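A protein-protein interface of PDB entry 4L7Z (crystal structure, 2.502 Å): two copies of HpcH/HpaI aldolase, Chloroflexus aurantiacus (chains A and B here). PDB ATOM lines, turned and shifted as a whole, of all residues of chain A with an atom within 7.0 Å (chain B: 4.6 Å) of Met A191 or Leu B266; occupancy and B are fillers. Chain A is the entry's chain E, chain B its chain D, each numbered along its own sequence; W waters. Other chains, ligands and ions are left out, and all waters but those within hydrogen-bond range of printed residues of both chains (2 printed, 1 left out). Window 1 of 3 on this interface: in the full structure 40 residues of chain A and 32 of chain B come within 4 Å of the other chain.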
ATOM      1  N   PRO A 182     -20.449   2.497 -28.807  1.00  0.00           N
ATOM      2  CA  PRO A 182     -19.114   2.999 -28.463  1.00  0.00           C
ATOM      3  C   PRO A 182     -18.375   2.118 -27.464  1.00  0.00           C
ATOM      4  O   PRO A 182     -17.217   1.777 -27.698  1.00  0.00           O
ATOM      5  CB  PRO A 182     -19.404   4.370 -27.836  1.00  0.00           C
ATOM      6  CG  PRO A 182     -20.780   4.729 -28.299  1.00  0.00           C
ATOM      7  CD  PRO A 182     -21.504   3.428 -28.373  1.00  0.00           C
ATOM      8  N   ALA A 183     -19.037   1.759 -26.371  1.00  0.00           N
ATOM      9  CA  ALA A 183     -18.411   0.957 -25.328  1.00  0.00           C
ATOM     10  C   ALA A 183     -18.015  -0.422 -25.842  1.00  0.00           C
ATOM     11  O   ALA A 183     -16.896  -0.881 -25.619  1.00  0.00           O
ATOM     12  CB  ALA A 183     -19.338   0.829 -24.129  1.00  0.00           C
ATOM     13  N   LEU A 185     -17.732  -1.494 -29.040  1.00  0.00           N
ATOM     14  CA  LEU A 185     -16.787  -1.428 -30.147  1.00  0.00           C
ATOM     15  C   LEU A 185     -15.376  -1.128 -29.649  1.00  0.00           C
ATOM     16  O   LEU A 185     -14.396  -1.662 -30.171  1.00  0.00           O
ATOM     17  CB  LEU A 185     -17.218  -0.379 -31.175  1.00  0.00           C
ATOM     18  CG  LEU A 185     -16.325  -0.278 -32.414  1.00  0.00           C
ATOM     19  CD1 LEU A 185     -16.288  -1.603 -33.156  1.00  0.00           C
ATOM     20  CD2 LEU A 185     -16.785   0.835 -33.335  1.00  0.00           C
ATOM     21  N   ALA A 186     -15.281  -0.273 -28.635  1.00  0.00           N
ATOM     22  CA  ALA A 186     -13.992   0.070 -28.044  1.00  0.00           C
ATOM     23  C   ALA A 186     -13.365  -1.154 -27.385  1.00  0.00           C
ATOM     24  O   ALA A 186     -12.160  -1.383 -27.496  1.00  0.00           O
ATOM     25  CB  ALA A 186     -14.149   1.197 -27.036  1.00  0.00           C
ATOM     26  N   ALA A 187     -14.195  -1.937 -26.703  1.00  0.00           N
ATOM     27  CA  ALA A 187     -13.736  -3.156 -26.051  1.00  0.00           C
ATOM     28  C   ALA A 187     -13.248  -4.174 -27.077  1.00  0.00           C
ATOM     29  O   ALA A 187     -12.253  -4.864 -26.855  1.00  0.00           O
ATOM     30  CB  ALA A 187     -14.844  -3.751 -25.199  1.00  0.00           C
ATOM     31  N   SER A 188     -13.954  -4.259 -28.201  1.00  0.00           N
ATOM     32  CA  SER A 188     -13.589  -5.178 -29.274  1.00  0.00           C
ATOM     33  C   SER A 188     -12.266  -4.780 -29.919  1.00  0.00           C
ATOM     34  O   SER A 188     -11.349  -5.593 -30.032  1.00  0.00           O
ATOM     35  CB  SER A 188     -14.691  -5.235 -30.336  1.00  0.00           C
ATOM     36  OG  SER A 188     -14.295  -6.028 -31.443  1.00  0.00           O
ATOM     37  N   ARG A 189     -12.177  -3.521 -30.339  1.00  0.00           N
ATOM     38  CA  ARG A 189     -10.980  -3.002 -30.987  1.00  0.00           C
ATOM     39  C   ARG A 189      -9.786  -2.996 -30.041  1.00  0.00           C
ATOM     40  O   ARG A 189      -8.657  -3.267 -30.447  1.00  0.00           O
ATOM     41  CB  ARG A 189     -11.227  -1.581 -31.491  1.00  0.00           C
ATOM     42  CG  ARG A 189     -12.200  -1.477 -32.649  1.00  0.00           C
ATOM     43  CD  ARG A 189     -12.567  -0.026 -32.902  1.00  0.00           C
ATOM     44  NE  ARG A 189     -13.152   0.178 -34.223  1.00  0.00           N
ATOM     45  CZ  ARG A 189     -13.613   1.345 -34.658  1.00  0.00           C
ATOM     46  NH1 ARG A 189     -13.566   2.413 -33.874  1.00  0.00           N
ATOM     47  NH2 ARG A 189     -14.128   1.445 -35.877  1.00  0.00           N
ATOM     48  N   GLY A 190     -10.045  -2.682 -28.777  1.00  0.00           N
ATOM     49  CA  GLY A 190      -8.983  -2.525 -27.805  1.00  0.00           C
ATOM     50  C   GLY A 190      -8.714  -1.054 -27.562  1.00  0.00           C
ATOM     51  O   GLY A 190      -7.666  -0.679 -27.036  1.00  0.00           O
ATOM     52  N   MET A 191      -9.667  -0.218 -27.964  1.00  0.00           N
ATOM     53  CA  MET A 191      -9.587   1.214 -27.710  1.00  0.00           C
ATOM     54  C   MET A 191      -9.630   1.497 -26.215  1.00  0.00           C
ATOM     55  O   MET A 191     -10.428   0.903 -25.486  1.00  0.00           O
ATOM     56  CB  MET A 191     -10.750   1.951 -28.378  1.00  0.00           C
ATOM     57  CG  MET A 191     -10.713   1.968 -29.892  1.00  0.00           C
ATOM     58  SD  MET A 191     -12.149   2.831 -30.560  1.00  0.00           S
ATOM     59  CE  MET A 191     -11.984   4.437 -29.785  1.00  0.00           C
ATOM     60  N   LYS A 192      -8.769   2.399 -25.756  1.00  0.00           N
ATOM     61  CA  LYS A 192      -8.836   2.868 -24.376  1.00  0.00           C
ATOM     62  C   LYS A 192      -9.661   4.145 -24.327  1.00  0.00           C
ATOM     63  O   LYS A 192      -9.238   5.189 -24.833  1.00  0.00           O
ATOM     64  CB  LYS A 192      -7.441   3.124 -23.803  1.00  0.00           C
ATOM     65  CG  LYS A 192      -6.506   1.929 -23.868  1.00  0.00           C
ATOM     66  CD  LYS A 192      -7.106   0.714 -23.187  1.00  0.00           C
ATOM     67  CE  LYS A 192      -6.318  -0.536 -23.526  1.00  0.00           C
ATOM     68  NZ  LYS A 192      -6.112  -0.664 -24.991  1.00  0.00           N
ATOM     69  N   THR A 193     -10.847   4.054 -23.735  1.00  0.00           N
ATOM     70  CA  THR A 193     -11.746   5.197 -23.646  1.00  0.00           C
ATOM     71  C   THR A 193     -12.205   5.419 -22.212  1.00  0.00           C
ATOM     72  O   THR A 193     -12.425   4.466 -21.463  1.00  0.00           O
ATOM     73  CB  THR A 193     -12.992   5.003 -24.528  1.00  0.00           C
ATOM     74  OG1 THR A 193     -13.747   3.883 -24.050  1.00  0.00           O
ATOM     75  CG2 THR A 193     -12.594   4.765 -25.978  1.00  0.00           C
ATOM     76  N   GLY A 198     -17.753   8.531 -24.912  1.00  0.00           N
ATOM     77  CA  GLY A 198     -16.716   9.545 -24.935  1.00  0.00           C
ATOM     78  C   GLY A 198     -15.434   9.050 -25.573  1.00  0.00           C
ATOM     79  O   GLY A 198     -15.372   7.928 -26.074  1.00  0.00           O
ATOM     80  N   GLY A 199     -14.408   9.894 -25.554  1.00  0.00           N
ATOM     81  CA  GLY A 199     -13.113   9.533 -26.098  1.00  0.00           C
ATOM     82  C   GLY A 199     -12.093   9.273 -25.008  1.00  0.00           C
ATOM     83  O   GLY A 199     -12.362   8.545 -24.052  1.00  0.00           O
ATOM     84  N   HIS A 200     -10.913   9.868 -25.154  1.00  0.00           N
ATOM     85  CA  HIS A 200      -9.862   9.753 -24.150  1.00  0.00           C
ATOM     86  C   HIS A 200      -9.022  11.027 -24.130  1.00  0.00           C
ATOM     87  O   HIS A 200      -8.585  11.501 -25.179  1.00  0.00           O
ATOM     88  CB  HIS A 200      -8.977   8.536 -24.425  1.00  0.00           C
ATOM     89  CG  HIS A 200      -8.182   8.088 -23.239  1.00  0.00           C
ATOM     90  ND1 HIS A 200      -7.059   8.757 -22.799  1.00  0.00           N
ATOM     91  CD2 HIS A 200      -8.347   7.038 -22.399  1.00  0.00           C
ATOM     92  CE1 HIS A 200      -6.567   8.139 -21.739  1.00  0.00           C
ATOM     93  NE2 HIS A 200      -7.329   7.092 -21.478  1.00  0.00           N
ATOM     94  N   TYR A 203      -5.441  11.187 -25.856  1.00  0.00           N
ATOM     95  CA  TYR A 203      -5.294  11.050 -27.299  1.00  0.00           C
ATOM     96  C   TYR A 203      -5.168  12.425 -27.937  1.00  0.00           C
ATOM     97  O   TYR A 203      -6.149  13.160 -28.052  1.00  0.00           O
ATOM     98  CB  TYR A 203      -6.471  10.283 -27.907  1.00  0.00           C
ATOM     99  CG  TYR A 203      -6.372  10.105 -29.405  1.00  0.00           C
ATOM    100  CD1 TYR A 203      -5.190   9.672 -29.996  1.00  0.00           C
ATOM    101  CD2 TYR A 203      -7.460  10.361 -30.232  1.00  0.00           C
ATOM    102  CE1 TYR A 203      -5.091   9.505 -31.365  1.00  0.00           C
ATOM    103  CE2 TYR A 203      -7.373  10.192 -31.604  1.00  0.00           C
ATOM    104  CZ  TYR A 203      -6.185   9.766 -32.164  1.00  0.00           C
ATOM    105  OH  TYR A 203      -6.086   9.599 -33.526  1.00  0.00           O
ATOM    106  N   ASP A 222     -10.003  13.497 -31.790  1.00  0.00           N
ATOM    107  CA  ASP A 222     -11.246  12.736 -31.722  1.00  0.00           C
ATOM    108  C   ASP A 222     -10.984  11.269 -32.053  1.00  0.00           C
ATOM    109  O   ASP A 222     -10.503  10.944 -33.139  1.00  0.00           O
ATOM    110  CB  ASP A 222     -12.276  13.323 -32.692  1.00  0.00           C
ATOM    111  CG  ASP A 222     -13.677  12.770 -32.477  1.00  0.00           C
ATOM    112  OD1 ASP A 222     -13.821  11.678 -31.888  1.00  0.00           O
ATOM    113  OD2 ASP A 222     -14.642  13.435 -32.911  1.00  0.00           O
ATOM    114  N   LEU A 223     -11.309  10.390 -31.110  1.00  0.00           N
ATOM    115  CA  LEU A 223     -11.112   8.955 -31.288  1.00  0.00           C
ATOM    116  C   LEU A 223     -12.030   8.365 -32.355  1.00  0.00           C
ATOM    117  O   LEU A 223     -11.651   7.430 -33.061  1.00  0.00           O
ATOM    118  CB  LEU A 223     -11.344   8.217 -29.967  1.00  0.00           C
ATOM    119  CG  LEU A 223     -10.189   8.120 -28.970  1.00  0.00           C
ATOM    120  CD1 LEU A 223     -10.653   7.456 -27.686  1.00  0.00           C
ATOM    121  CD2 LEU A 223      -9.037   7.343 -29.572  1.00  0.00           C
ATOM    122  N   TRP A 224     -13.234   8.918 -32.470  1.00  0.00           N
ATOM    123  CA  TRP A 224     -14.290   8.293 -33.262  1.00  0.00           C
ATOM    124  C   TRP A 224     -14.469   8.855 -34.672  1.00  0.00           C
ATOM    125  O   TRP A 224     -15.447   8.530 -35.345  1.00  0.00           O
ATOM    126  CB  TRP A 224     -15.623   8.372 -32.513  1.00  0.00           C
ATOM    127  CG  TRP A 224     -15.622   7.654 -31.200  1.00  0.00           C
ATOM    128  CD1 TRP A 224     -15.555   8.215 -29.959  1.00  0.00           C
ATOM    129  CD2 TRP A 224     -15.688   6.237 -30.999  1.00  0.00           C
ATOM    130  NE1 TRP A 224     -15.578   7.235 -28.996  1.00  0.00           N
ATOM    131  CE2 TRP A 224     -15.658   6.013 -29.608  1.00  0.00           C
ATOM    132  CE3 TRP A 224     -15.769   5.138 -31.859  1.00  0.00           C
ATOM    133  CZ2 TRP A 224     -15.707   4.733 -29.058  1.00  0.00           C
ATOM    134  CZ3 TRP A 224     -15.817   3.870 -31.311  1.00  0.00           C
ATOM    135  CH2 TRP A 224     -15.786   3.677 -29.925  1.00  0.00           C
ATOM    136  N   THR A 227     -14.449   6.179 -37.441  1.00  0.00           N
ATOM    137  CA  THR A 227     -15.583   5.281 -37.271  1.00  0.00           C
ATOM    138  C   THR A 227     -16.882   5.883 -37.800  1.00  0.00           C
ATOM    139  O   THR A 227     -17.594   5.249 -38.579  1.00  0.00           O
ATOM    140  CB  THR A 227     -15.761   4.888 -35.795  1.00  0.00           C
ATOM    141  OG1 THR A 227     -14.592   4.191 -35.344  1.00  0.00           O
ATOM    142  CG2 THR A 227     -16.976   3.991 -35.621  1.00  0.00           C
ATOM    143  N   HIS B 225      -4.361   9.229 -37.939  1.00  0.00           N
ATOM    144  CA  HIS B 225      -5.630   8.727 -37.413  1.00  0.00           C
ATOM    145  C   HIS B 225      -6.255   7.669 -38.320  1.00  0.00           C
ATOM    146  O   HIS B 225      -6.488   6.537 -37.893  1.00  0.00           O
ATOM    147  CB  HIS B 225      -6.618   9.874 -37.190  1.00  0.00           C
ATOM    148  CG  HIS B 225      -7.950   9.427 -36.674  1.00  0.00           C
ATOM    149  ND1 HIS B 225      -8.116   8.883 -35.419  1.00  0.00           N
ATOM    150  CD2 HIS B 225      -9.177   9.433 -37.247  1.00  0.00           C
ATOM    151  CE1 HIS B 225      -9.389   8.578 -35.238  1.00  0.00           C
ATOM    152  NE2 HIS B 225     -10.054   8.900 -36.333  1.00  0.00           N
ATOM    153  N   ILE B 228      -3.980   4.322 -38.576  1.00  0.00           N
ATOM    154  CA  ILE B 228      -3.996   3.429 -37.422  1.00  0.00           C
ATOM    155  C   ILE B 228      -5.373   2.806 -37.212  1.00  0.00           C
ATOM    156  O   ILE B 228      -5.487   1.600 -36.986  1.00  0.00           O
ATOM    157  CB  ILE B 228      -3.562   4.152 -36.132  1.00  0.00           C
ATOM    158  CG1 ILE B 228      -2.144   4.707 -36.282  1.00  0.00           C
ATOM    159  CG2 ILE B 228      -3.637   3.207 -34.941  1.00  0.00           C
ATOM    160  CD1 ILE B 228      -1.645   5.450 -35.059  1.00  0.00           C
ATOM    161  N   VAL B 232      -6.073  -1.127 -37.166  1.00  0.00           N
ATOM    162  CA  VAL B 232      -6.612  -1.834 -36.007  1.00  0.00           C
ATOM    163  C   VAL B 232      -7.824  -2.693 -36.368  1.00  0.00           C
ATOM    164  O   VAL B 232      -7.869  -3.880 -36.039  1.00  0.00           O
ATOM    165  CB  VAL B 232      -6.996  -0.861 -34.870  1.00  0.00           C
ATOM    166  CG1 VAL B 232      -7.743  -1.596 -33.766  1.00  0.00           C
ATOM    167  CG2 VAL B 232      -5.759  -0.179 -34.311  1.00  0.00           C
ATOM    168  N   ASN B 262      -0.909   7.263 -28.297  1.00  0.00           N
ATOM    169  CA  ASN B 262      -1.984   7.373 -29.279  1.00  0.00           C
ATOM    170  C   ASN B 262      -2.274   6.042 -29.965  1.00  0.00           C
ATOM    171  O   ASN B 262      -3.430   5.704 -30.222  1.00  0.00           O
ATOM    172  CB  ASN B 262      -1.658   8.440 -30.326  1.00  0.00           C
ATOM    173  CG  ASN B 262      -1.689   9.843 -29.758  1.00  0.00           C
ATOM    174  OD1 ASN B 262      -2.344  10.102 -28.749  1.00  0.00           O
ATOM    175  ND2 ASN B 262      -0.985  10.760 -30.410  1.00  0.00           N
ATOM    176  N   ALA B 263      -1.217   5.290 -30.258  1.00  0.00           N
ATOM    177  CA  ALA B 263      -1.363   3.970 -30.857  1.00  0.00           C
ATOM    178  C   ALA B 263      -2.032   3.014 -29.876  1.00  0.00           C
ATOM    179  O   ALA B 263      -2.908   2.234 -30.250  1.00  0.00           O
ATOM    180  CB  ALA B 263      -0.008   3.430 -31.287  1.00  0.00           C
ATOM    181  N   PHE B 264      -1.616   3.090 -28.616  1.00  0.00           N
ATOM    182  CA  PHE B 264      -2.165   2.245 -27.563  1.00  0.00           C
ATOM    183  C   PHE B 264      -3.649   2.523 -27.335  1.00  0.00           C
ATOM    184  O   PHE B 264      -4.441   1.598 -27.143  1.00  0.00           O
ATOM    185  CB  PHE B 264      -1.384   2.450 -26.264  1.00  0.00           C
ATOM    186  CG  PHE B 264      -1.915   1.661 -25.101  1.00  0.00           C
ATOM    187  CD1 PHE B 264      -1.752   0.287 -25.045  1.00  0.00           C
ATOM    188  CD2 PHE B 264      -2.564   2.297 -24.055  1.00  0.00           C
ATOM    189  CE1 PHE B 264      -2.235  -0.440 -23.973  1.00  0.00           C
ATOM    190  CE2 PHE B 264      -3.049   1.576 -22.980  1.00  0.00           C
ATOM    191  CZ  PHE B 264      -2.883   0.206 -22.939  1.00  0.00           C
ATOM    192  N   LEU B 265      -4.021   3.799 -27.363  1.00  0.00           N
ATOM    193  CA  LEU B 265      -5.409   4.194 -27.149  1.00  0.00           C
ATOM    194  C   LEU B 265      -6.299   3.767 -28.313  1.00  0.00           C
ATOM    195  O   LEU B 265      -7.512   3.625 -28.157  1.00  0.00           O
ATOM    196  CB  LEU B 265      -5.516   5.706 -26.933  1.00  0.00           C
ATOM    197  CG  LEU B 265      -4.726   6.306 -25.764  1.00  0.00           C
ATOM    198  CD1 LEU B 265      -4.914   7.811 -25.702  1.00  0.00           C
ATOM    199  CD2 LEU B 265      -5.114   5.668 -24.443  1.00  0.00           C
ATOM    200  N   LEU B 266      -5.695   3.562 -29.480  1.00  0.00           N
ATOM    201  CA  LEU B 266      -6.445   3.156 -30.665  1.00  0.00           C
ATOM    202  C   LEU B 266      -6.514   1.638 -30.823  1.00  0.00           C
ATOM    203  O   LEU B 266      -7.249   1.130 -31.667  1.00  0.00           O
ATOM    204  CB  LEU B 266      -5.864   3.803 -31.927  1.00  0.00           C
ATOM    205  CG  LEU B 266      -6.213   5.281 -32.121  1.00  0.00           C
ATOM    206  CD1 LEU B 266      -5.475   5.870 -33.311  1.00  0.00           C
ATOM    207  CD2 LEU B 266      -7.710   5.446 -32.293  1.00  0.00           C
ATOM    208  N   GLY B 267      -5.747   0.918 -30.010  1.00  0.00           N
ATOM    209  CA  GLY B 267      -5.833  -0.531 -29.985  1.00  0.00           C
ATOM    210  C   GLY B 267      -4.574  -1.281 -30.380  1.00  0.00           C
ATOM    211  O   GLY B 267      -4.611  -2.497 -30.565  1.00  0.00           O
ATOM    212  N   CYS B 268      -3.459  -0.570 -30.512  1.00  0.00           N
ATOM    213  CA  CYS B 268      -2.199  -1.217 -30.871  1.00  0.00           C
ATOM    214  C   CYS B 268      -1.616  -2.006 -29.701  1.00  0.00           C
ATOM    215  O   CYS B 268      -1.775  -1.626 -28.541  1.00  0.00           O
ATOM    216  CB  CYS B 268      -1.184  -0.198 -31.393  1.00  0.00           C
ATOM    217  SG  CYS B 268      -1.581   0.468 -33.026  1.00  0.00           S
HETATM  218  O   HOH W   1      -3.905  -1.622 -26.836  1.00  0.00           O
HETATM  219  O   HOH W   2      -9.567   2.071 -32.967  1.00  0.00           O
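A ring nitrogen (ND1) of His B225 is in hydrogen-bond range of the side-chain hydroxyl (OH) of Tyr A203, 2.9 Å away. O of Leu B265 sits at hydrogen-bond distance from N of Lys A192 (3.0 Å).
Water W1 lies within hydrogen-bond range of the backbone carbonyl oxygen (O) of Cys B268 (2.7 Å), the side-chain amino group (NZ) of Lys A192 (3.0 Å) and the backbone carbonyl oxygen (O) of Phe B264 (3.3 Å). Water W2 bridges O of Leu B266 (2.8 Å) and SD of Met A191 (3.6 Å).
O of Ala A186 lies within hydrogen-bond range of N of Met A191 (2.8 Å). The side-chain sulfur (SD) of Met A191 lies within hydrogen-bond range of the guanidinium group (NH1) of Arg A189 (3.6 Å). The guanidinium group (NH1) of Arg A189 sits at hydrogen-bond distance from the side-chain hydroxyl (OG1) of Thr A227. The side-chain amino group of Lys A192 sits at hydrogen-bond distance from the backbone carbonyl oxygen of Gly A190 (2.6 Å). The side-chain carboxylate of Asp A222 is in hydrogen-bond range of the backbone NH of Trp A224, at 2.9 Å.
Printed residues of chain A that touch a printed residue of chain B: Arg A189, Gly A190, Met A191, Lys A192, His A200, Tyr A203, Asp A222 and Leu A223. Among the printed residues, 16 pairs touch across the chains. Among the printed residues, no Asp or Glu carboxylate lies within 4 Å of a Lys or Arg side-chain nitrogen of the other chain.
Among the printed residues, merely in contact across the chains: Tyr A203 with Asn B262 (3.1 Å), Met A191 with Leu B265 (3.2 Å), Leu A223 with His B225 (3.3 Å), Asp A222 with His B225 (3.4 Å), Tyr A203 with Leu B265 (3.4 Å), Gly A190 with Gly B267 (3.5 Å), Lys A192 with Phe B264 (3.5 Å), Leu A223 with Leu B266 (3.6 Å), His A200 with Leu B265 (3.7 Å), Tyr A203 with Leu B266 (3.8 Å), Arg A189 with Val B232 (3.8 Å), Gly A190 with Phe B264 (3.9 Å), Arg A189 with Gly B267 (3.96 Å) and Met A191 with Leu B266 (3.98 Å).
No position is printed for both chains.
Of the printed residues of chain B, Met A191 touches Leu B265 (3.2 Å) and Leu B266 (3.98 Å). Of the printed residues of chain B, Tyr A203 touches His B225, Asn B262, Leu B265 and Leu B266. Printed residues of chain B within 4 Å of His A200: Leu B265. Trp A224 touches none of the printed residues of chain B.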
